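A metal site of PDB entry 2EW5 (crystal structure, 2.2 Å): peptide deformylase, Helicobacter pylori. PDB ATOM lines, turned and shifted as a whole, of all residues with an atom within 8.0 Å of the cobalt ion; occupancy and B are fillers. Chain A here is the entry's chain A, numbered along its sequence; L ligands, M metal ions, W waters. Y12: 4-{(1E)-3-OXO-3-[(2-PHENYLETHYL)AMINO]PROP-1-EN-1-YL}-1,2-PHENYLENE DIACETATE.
N9 of the ligand is in hydrogen-bond range of O of Gly 94, at 3.1 Å. The backbone NH (N) of Gly 45 lies within hydrogen-bond range of an oxygen (O27) of the ligand, at 3.4 Å.
NE2 of Gln 50 touches the cobalt ion (3.4 Å). OE2 of Glu 138 touches the cobalt ion, at 3.9 Å. The nearest printed residue that does not touch the cobalt ion is Leu 96 (4.7 Å).
A ring nitrogen (ND1) of His 137 lies within hydrogen-bond range of the side-chain carboxylate (OE1) of Glu 93. The side-chain amide nitrogen (NE2) of Gln 50 sits close to the side-chain sulfur (SG) of Cys 95 (3.4 Å). The side-chain sulfur (SG) of Cys 95 lies close to the backbone NH (N) of Ser 97, at 3.4 Å. The side-chain amide nitrogen (NE2) of Gln 50 is in hydrogen-bond range of the side-chain hydroxyl (OG) of Ser 97. N of Ala 47 sits at hydrogen-bond distance from OE1 of Gln 50 (2.8 Å). The side-chain carboxylate (OE1) of Glu 138 lies within hydrogen-bond range of the backbone NH (N) of Ala 47 (3.1 Å).
Water W1 bridges the side-chain carboxylate (OE2) of Glu 138 and the side-chain amide oxygen (OE1) of Gln 50.
Water W1 is bound to the cobalt ion, 2.0 Å away. NE2 of His 141 binds the cobalt ion (2.2 Å). NE2 of His 137 is bound to the cobalt ion (2.2 Å). The cobalt ion is bound by SG of Cys 95 (2.4 Å). The cobalt ion has four donor atoms within binding distance.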
ATOM      1  N   LEU A  13      32.364  10.273   3.532  1.00  0.00           N
ATOM      2  CA  LEU A  13      31.017   9.752   3.312  1.00  0.00           C
ATOM      3  C   LEU A  13      30.346   9.269   4.598  1.00  0.00           C
ATOM      4  O   LEU A  13      29.182   8.859   4.584  1.00  0.00           O
ATOM      5  CB  LEU A  13      31.047   8.629   2.275  1.00  0.00           C
ATOM      6  CG  LEU A  13      31.575   9.035   0.886  1.00  0.00           C
ATOM      7  CD1 LEU A  13      31.801   7.811   0.039  1.00  0.00           C
ATOM      8  CD2 LEU A  13      30.587   9.975   0.212  1.00  0.00           C
ATOM      9  N   GLY A  45      20.443  10.324  -8.698  1.00  0.00           N
ATOM     10  CA  GLY A  45      20.348  10.832  -7.341  1.00  0.00           C
ATOM     11  C   GLY A  45      21.724  11.301  -6.859  1.00  0.00           C
ATOM     12  O   GLY A  45      22.741  10.745  -7.261  1.00  0.00           O
ATOM     13  N   LEU A  46      21.753  12.325  -6.020  1.00  0.00           N
ATOM     14  CA  LEU A  46      23.022  12.828  -5.491  1.00  0.00           C
ATOM     15  C   LEU A  46      22.806  13.609  -4.192  1.00  0.00           C
ATOM     16  O   LEU A  46      21.965  14.508  -4.129  1.00  0.00           O
ATOM     17  CB  LEU A  46      23.706  13.752  -6.514  1.00  0.00           C
ATOM     18  CG  LEU A  46      25.116  14.223  -6.141  1.00  0.00           C
ATOM     19  CD1 LEU A  46      26.076  13.049  -6.216  1.00  0.00           C
ATOM     20  CD2 LEU A  46      25.584  15.323  -7.087  1.00  0.00           C
ATOM     21  N   ALA A  47      23.563  13.254  -3.161  1.00  0.00           N
ATOM     22  CA  ALA A  47      23.469  13.920  -1.865  1.00  0.00           C
ATOM     23  C   ALA A  47      24.625  14.909  -1.755  1.00  0.00           C
ATOM     24  O   ALA A  47      25.690  14.702  -2.347  1.00  0.00           O
ATOM     25  CB  ALA A  47      23.548  12.892  -0.747  1.00  0.00           C
ATOM     26  N   ILE A  49      26.897  15.528   0.563  1.00  0.00           N
ATOM     27  CA  ILE A  49      28.202  15.008   0.987  1.00  0.00           C
ATOM     28  C   ILE A  49      28.966  14.279  -0.118  1.00  0.00           C
ATOM     29  O   ILE A  49      30.178  14.135  -0.026  1.00  0.00           O
ATOM     30  CB  ILE A  49      28.140  14.052   2.203  1.00  0.00           C
ATOM     31  CG1 ILE A  49      26.759  13.412   2.301  1.00  0.00           C
ATOM     32  CG2 ILE A  49      28.570  14.777   3.453  1.00  0.00           C
ATOM     33  CD1 ILE A  49      26.483  12.407   1.206  1.00  0.00           C
ATOM     34  N   GLN A  50      28.262  13.815  -1.141  1.00  0.00           N
ATOM     35  CA  GLN A  50      28.925  13.116  -2.234  1.00  0.00           C
ATOM     36  C   GLN A  50      29.814  14.089  -3.023  1.00  0.00           C
ATOM     37  O   GLN A  50      30.612  13.662  -3.863  1.00  0.00           O
ATOM     38  CB  GLN A  50      27.900  12.452  -3.162  1.00  0.00           C
ATOM     39  CG  GLN A  50      27.302  11.180  -2.572  1.00  0.00           C
ATOM     40  CD  GLN A  50      26.288  10.522  -3.494  1.00  0.00           C
ATOM     41  OE1 GLN A  50      25.119  10.941  -3.561  1.00  0.00           O
ATOM     42  NE2 GLN A  50      26.720   9.492  -4.217  1.00  0.00           N
ATOM     43  N   GLU A  93      20.466  -1.640  -6.075  1.00  0.00           N
ATOM     44  CA  GLU A  93      20.898  -0.260  -6.071  1.00  0.00           C
ATOM     45  C   GLU A  93      22.313  -0.021  -6.583  1.00  0.00           C
ATOM     46  O   GLU A  93      23.147  -0.925  -6.596  1.00  0.00           O
ATOM     47  CB  GLU A  93      20.776   0.306  -4.650  1.00  0.00           C
ATOM     48  CG  GLU A  93      19.360   0.328  -4.117  1.00  0.00           C
ATOM     49  CD  GLU A  93      19.249   1.004  -2.756  1.00  0.00           C
ATOM     50  OE1 GLU A  93      20.118   1.840  -2.420  1.00  0.00           O
ATOM     51  OE2 GLU A  93      18.275   0.720  -2.034  1.00  0.00           O
ATOM     52  N   GLY A  94      22.555   1.219  -6.996  1.00  0.00           N
ATOM     53  CA  GLY A  94      23.856   1.645  -7.486  1.00  0.00           C
ATOM     54  C   GLY A  94      24.107   3.000  -6.862  1.00  0.00           C
ATOM     55  O   GLY A  94      23.189   3.599  -6.325  1.00  0.00           O
ATOM     56  N   CYS A  95      25.336   3.508  -6.940  1.00  0.00           N
ATOM     57  CA  CYS A  95      25.661   4.802  -6.324  1.00  0.00           C
ATOM     58  C   CYS A  95      26.900   5.437  -6.988  1.00  0.00           C
ATOM     59  O   CYS A  95      27.875   4.742  -7.277  1.00  0.00           O
ATOM     60  CB  CYS A  95      25.936   4.599  -4.831  1.00  0.00           C
ATOM     61  SG  CYS A  95      26.292   6.103  -3.863  1.00  0.00           S
ATOM     62  N   LEU A  96      26.828   6.746  -7.229  1.00  0.00           N
ATOM     63  CA  LEU A  96      27.934   7.480  -7.838  1.00  0.00           C
ATOM     64  C   LEU A  96      29.183   7.438  -6.965  1.00  0.00           C
ATOM     65  O   LEU A  96      30.306   7.611  -7.452  1.00  0.00           O
ATOM     66  CB  LEU A  96      27.543   8.949  -8.080  1.00  0.00           C
ATOM     67  CG  LEU A  96      26.607   9.217  -9.254  1.00  0.00           C
ATOM     68  CD1 LEU A  96      26.139  10.654  -9.250  1.00  0.00           C
ATOM     69  CD2 LEU A  96      27.340   8.922 -10.527  1.00  0.00           C
ATOM     70  N   SER A  97      29.004   7.190  -5.672  1.00  0.00           N
ATOM     71  CA  SER A  97      30.151   7.136  -4.772  1.00  0.00           C
ATOM     72  C   SER A  97      30.684   5.713  -4.631  1.00  0.00           C
ATOM     73  O   SER A  97      31.634   5.471  -3.891  1.00  0.00           O
ATOM     74  CB  SER A  97      29.776   7.703  -3.400  1.00  0.00           C
ATOM     75  OG  SER A  97      29.555   9.102  -3.487  1.00  0.00           O
ATOM     76  N   VAL A  98      30.062   4.771  -5.332  1.00  0.00           N
ATOM     77  CA  VAL A  98      30.490   3.383  -5.307  1.00  0.00           C
ATOM     78  C   VAL A  98      30.301   2.898  -6.734  1.00  0.00           C
ATOM     79  O   VAL A  98      29.588   1.929  -6.997  1.00  0.00           O
ATOM     80  CB  VAL A  98      29.625   2.528  -4.368  1.00  0.00           C
ATOM     81  CG1 VAL A  98      30.281   1.157  -4.158  1.00  0.00           C
ATOM     82  CG2 VAL A  98      29.434   3.235  -3.032  1.00  0.00           C
ATOM     83  N   ARG A 107      14.400  -2.148   1.341  1.00  0.00           N
ATOM     84  CA  ARG A 107      13.881  -0.808   1.585  1.00  0.00           C
ATOM     85  C   ARG A 107      12.381  -0.852   1.869  1.00  0.00           C
ATOM     86  O   ARG A 107      11.735  -1.868   1.639  1.00  0.00           O
ATOM     87  CB  ARG A 107      14.086   0.069   0.342  1.00  0.00           C
ATOM     88  CG  ARG A 107      15.524   0.226  -0.120  1.00  0.00           C
ATOM     89  CD  ARG A 107      16.317   1.071   0.844  1.00  0.00           C
ATOM     90  NE  ARG A 107      17.608   1.443   0.285  1.00  0.00           N
ATOM     91  CZ  ARG A 107      18.493   2.211   0.906  1.00  0.00           C
ATOM     92  NH1 ARG A 107      18.226   2.705   2.110  1.00  0.00           N
ATOM     93  NH2 ARG A 107      19.661   2.491   0.321  1.00  0.00           N
ATOM     94  N   ALA A 134      14.952   5.830  -4.021  1.00  0.00           N
ATOM     95  CA  ALA A 134      15.929   6.898  -4.186  1.00  0.00           C
ATOM     96  C   ALA A 134      15.917   7.797  -2.966  1.00  0.00           C
ATOM     97  O   ALA A 134      16.966   8.192  -2.471  1.00  0.00           O
ATOM     98  CB  ALA A 134      15.612   7.711  -5.447  1.00  0.00           C
ATOM     99  N   HIS A 137      17.619   5.999  -0.095  1.00  0.00           N
ATOM    100  CA  HIS A 137      19.044   5.900  -0.400  1.00  0.00           C
ATOM    101  C   HIS A 137      19.711   7.252  -0.174  1.00  0.00           C
ATOM    102  O   HIS A 137      20.670   7.352   0.591  1.00  0.00           O
ATOM    103  CB  HIS A 137      19.229   5.458  -1.856  1.00  0.00           C
ATOM    104  CG  HIS A 137      20.655   5.372  -2.303  1.00  0.00           C
ATOM    105  ND1 HIS A 137      21.255   4.188  -2.648  1.00  0.00           N
ATOM    106  CD2 HIS A 137      21.580   6.338  -2.541  1.00  0.00           C
ATOM    107  CE1 HIS A 137      22.480   4.420  -3.086  1.00  0.00           C
ATOM    108  NE2 HIS A 137      22.703   5.713  -3.032  1.00  0.00           N
ATOM    109  N   GLU A 138      19.188   8.300  -0.800  1.00  0.00           N
ATOM    110  CA  GLU A 138      19.790   9.610  -0.640  1.00  0.00           C
ATOM    111  C   GLU A 138      19.796  10.094   0.812  1.00  0.00           C
ATOM    112  O   GLU A 138      20.816  10.607   1.291  1.00  0.00           O
ATOM    113  CB  GLU A 138      19.099  10.647  -1.525  1.00  0.00           C
ATOM    114  CG  GLU A 138      19.313  10.417  -3.025  1.00  0.00           C
ATOM    115  CD  GLU A 138      20.767  10.164  -3.383  1.00  0.00           C
ATOM    116  OE1 GLU A 138      21.655  10.791  -2.772  1.00  0.00           O
ATOM    117  OE2 GLU A 138      21.026   9.333  -4.287  1.00  0.00           O
ATOM    118  N   ILE A 139      18.675   9.921   1.518  1.00  0.00           N
ATOM    119  CA  ILE A 139      18.609  10.323   2.913  1.00  0.00           C
ATOM    120  C   ILE A 139      19.647   9.587   3.741  1.00  0.00           C
ATOM    121  O   ILE A 139      20.197  10.151   4.691  1.00  0.00           O
ATOM    122  CB  ILE A 139      17.176  10.127   3.489  1.00  0.00           C
ATOM    123  CG1 ILE A 139      16.285  11.287   3.015  1.00  0.00           C
ATOM    124  CG2 ILE A 139      17.212  10.107   5.010  1.00  0.00           C
ATOM    125  CD1 ILE A 139      14.825  11.122   3.365  1.00  0.00           C
ATOM    126  N   ASP A 140      19.920   8.328   3.395  1.00  0.00           N
ATOM    127  CA  ASP A 140      20.934   7.563   4.119  1.00  0.00           C
ATOM    128  C   ASP A 140      22.283   8.314   4.034  1.00  0.00           C
ATOM    129  O   ASP A 140      23.025   8.383   5.010  1.00  0.00           O
ATOM    130  CB  ASP A 140      21.097   6.152   3.536  1.00  0.00           C
ATOM    131  CG  ASP A 140      20.186   5.118   4.222  1.00  0.00           C
ATOM    132  OD1 ASP A 140      19.510   5.472   5.206  1.00  0.00           O
ATOM    133  OD2 ASP A 140      20.150   3.955   3.770  1.00  0.00           O
ATOM    134  N   HIS A 141      22.581   8.899   2.873  1.00  0.00           N
ATOM    135  CA  HIS A 141      23.820   9.648   2.723  1.00  0.00           C
ATOM    136  C   HIS A 141      23.949  10.771   3.745  1.00  0.00           C
ATOM    137  O   HIS A 141      25.037  11.012   4.264  1.00  0.00           O
ATOM    138  CB  HIS A 141      23.948  10.256   1.330  1.00  0.00           C
ATOM    139  CG  HIS A 141      24.473   9.302   0.302  1.00  0.00           C
ATOM    140  ND1 HIS A 141      25.674   8.648   0.445  1.00  0.00           N
ATOM    141  CD2 HIS A 141      23.970   8.901  -0.890  1.00  0.00           C
ATOM    142  CE1 HIS A 141      25.884   7.882  -0.620  1.00  0.00           C
ATOM    143  NE2 HIS A 141      24.859   8.021  -1.438  1.00  0.00           N
ATOM    144  N   VAL A 145      25.461   7.019   5.729  1.00  0.00           N
ATOM    145  CA  VAL A 145      25.188   5.613   5.419  1.00  0.00           C
ATOM    146  C   VAL A 145      25.210   5.320   3.917  1.00  0.00           C
ATOM    147  O   VAL A 145      24.554   6.014   3.140  1.00  0.00           O
ATOM    148  CB  VAL A 145      23.811   5.199   5.963  1.00  0.00           C
ATOM    149  CG1 VAL A 145      23.509   3.747   5.578  1.00  0.00           C
ATOM    150  CG2 VAL A 145      23.781   5.355   7.469  1.00  0.00           C
ATOM    151  N   LEU A 146      25.954   4.291   3.524  1.00  0.00           N
ATOM    152  CA  LEU A 146      26.047   3.878   2.128  1.00  0.00           C
ATOM    153  C   LEU A 146      25.256   2.589   1.964  1.00  0.00           C
ATOM    154  O   LEU A 146      25.159   1.805   2.908  1.00  0.00           O
ATOM    155  CB  LEU A 146      27.512   3.640   1.734  1.00  0.00           C
ATOM    156  CG  LEU A 146      28.481   4.795   1.948  1.00  0.00           C
ATOM    157  CD1 LEU A 146      29.880   4.356   1.535  1.00  0.00           C
ATOM    158  CD2 LEU A 146      28.032   6.009   1.143  1.00  0.00           C
ATOM    159  N   PHE A 147      24.690   2.354   0.778  1.00  0.00           N
ATOM    160  CA  PHE A 147      23.901   1.149   0.597  1.00  0.00           C
ATOM    161  C   PHE A 147      24.707  -0.132   0.788  1.00  0.00           C
ATOM    162  O   PHE A 147      24.130  -1.168   1.101  1.00  0.00           O
ATOM    163  CB  PHE A 147      23.197   1.142  -0.766  1.00  0.00           C
ATOM    164  CG  PHE A 147      24.080   0.772  -1.924  1.00  0.00           C
ATOM    165  CD1 PHE A 147      24.933   1.706  -2.497  1.00  0.00           C
ATOM    166  CD2 PHE A 147      24.038  -0.511  -2.457  1.00  0.00           C
ATOM    167  CE1 PHE A 147      25.722   1.365  -3.608  1.00  0.00           C
ATOM    168  CE2 PHE A 147      24.818  -0.859  -3.560  1.00  0.00           C
ATOM    169  CZ  PHE A 147      25.661   0.090  -4.133  1.00  0.00           C
HETATM  170  C2  Y12 L   1      17.709   3.225  -7.017  1.00  0.00           C
HETATM  171  C3  Y12 L   1      17.464   4.548  -7.475  1.00  0.00           C
HETATM  172  C4  Y12 L   1      18.328   5.615  -7.096  1.00  0.00           C
HETATM  173  C5  Y12 L   1      19.441   5.367  -6.245  1.00  0.00           C
HETATM  174  C7  Y12 L   1      20.373   6.526  -5.844  1.00  0.00           C
HETATM  175  C8  Y12 L   1      21.027   7.081  -7.116  1.00  0.00           C
HETATM  176  N9  Y12 L   1      22.145   6.254  -7.615  1.00  0.00           N
HETATM  177  C10 Y12 L   1      22.769   6.644  -8.768  1.00  0.00           C
HETATM  178  O27 Y12 L   1      22.392   7.670  -9.344  1.00  0.00           O
HETATM  179  C11 Y12 L   1      23.915   5.856  -9.326  1.00  0.00           C
HETATM  180  C12 Y12 L   1      24.580   6.198 -10.479  1.00  0.00           C
HETATM  181  C13 Y12 L   1      25.829   5.518 -11.075  1.00  0.00           C
HETATM  182  C18 Y12 L   1      26.605   6.178 -12.095  1.00  0.00           C
HETATM  183  C17 Y12 L   1      27.809   5.606 -12.621  1.00  0.00           C
HETATM  184  O23 Y12 L   1      28.531   6.321 -13.626  1.00  0.00           O
HETATM  185  C24 Y12 L   1      29.666   7.048 -13.336  1.00  0.00           C
HETATM  186  O26 Y12 L   1      30.188   7.180 -12.215  1.00  0.00           O
HETATM  187  C25 Y12 L   1      30.273   7.723 -14.532  1.00  0.00           C
HETATM  188  C16 Y12 L   1      28.268   4.339 -12.126  1.00  0.00           C
HETATM  189  O19 Y12 L   1      29.483   3.774 -12.631  1.00  0.00           O
HETATM  190  C20 Y12 L   1      29.487   2.847 -13.616  1.00  0.00           C
HETATM  191  O22 Y12 L   1      28.483   2.420 -14.170  1.00  0.00           O
HETATM  192  C21 Y12 L   1      30.845   2.361 -14.004  1.00  0.00           C
HETATM  193  C15 Y12 L   1      27.504   3.652 -11.112  1.00  0.00           C
HETATM  194  C14 Y12 L   1      26.294   4.248 -10.587  1.00  0.00           C
HETATM  195  C6  Y12 L   1      19.682   4.035  -5.771  1.00  0.00           C
HETATM  196  C1  Y12 L   1      18.811   2.971  -6.171  1.00  0.00           C
HETATM  197 CO    CO M   1      24.256   7.265  -3.365  1.00  0.00          CO
HETATM  198  O   HOH W   1      23.590   8.937  -4.285  1.00  0.00           O
HETATM  199  O   HOH W   2      24.928   4.701  -1.143  1.00  0.00           O
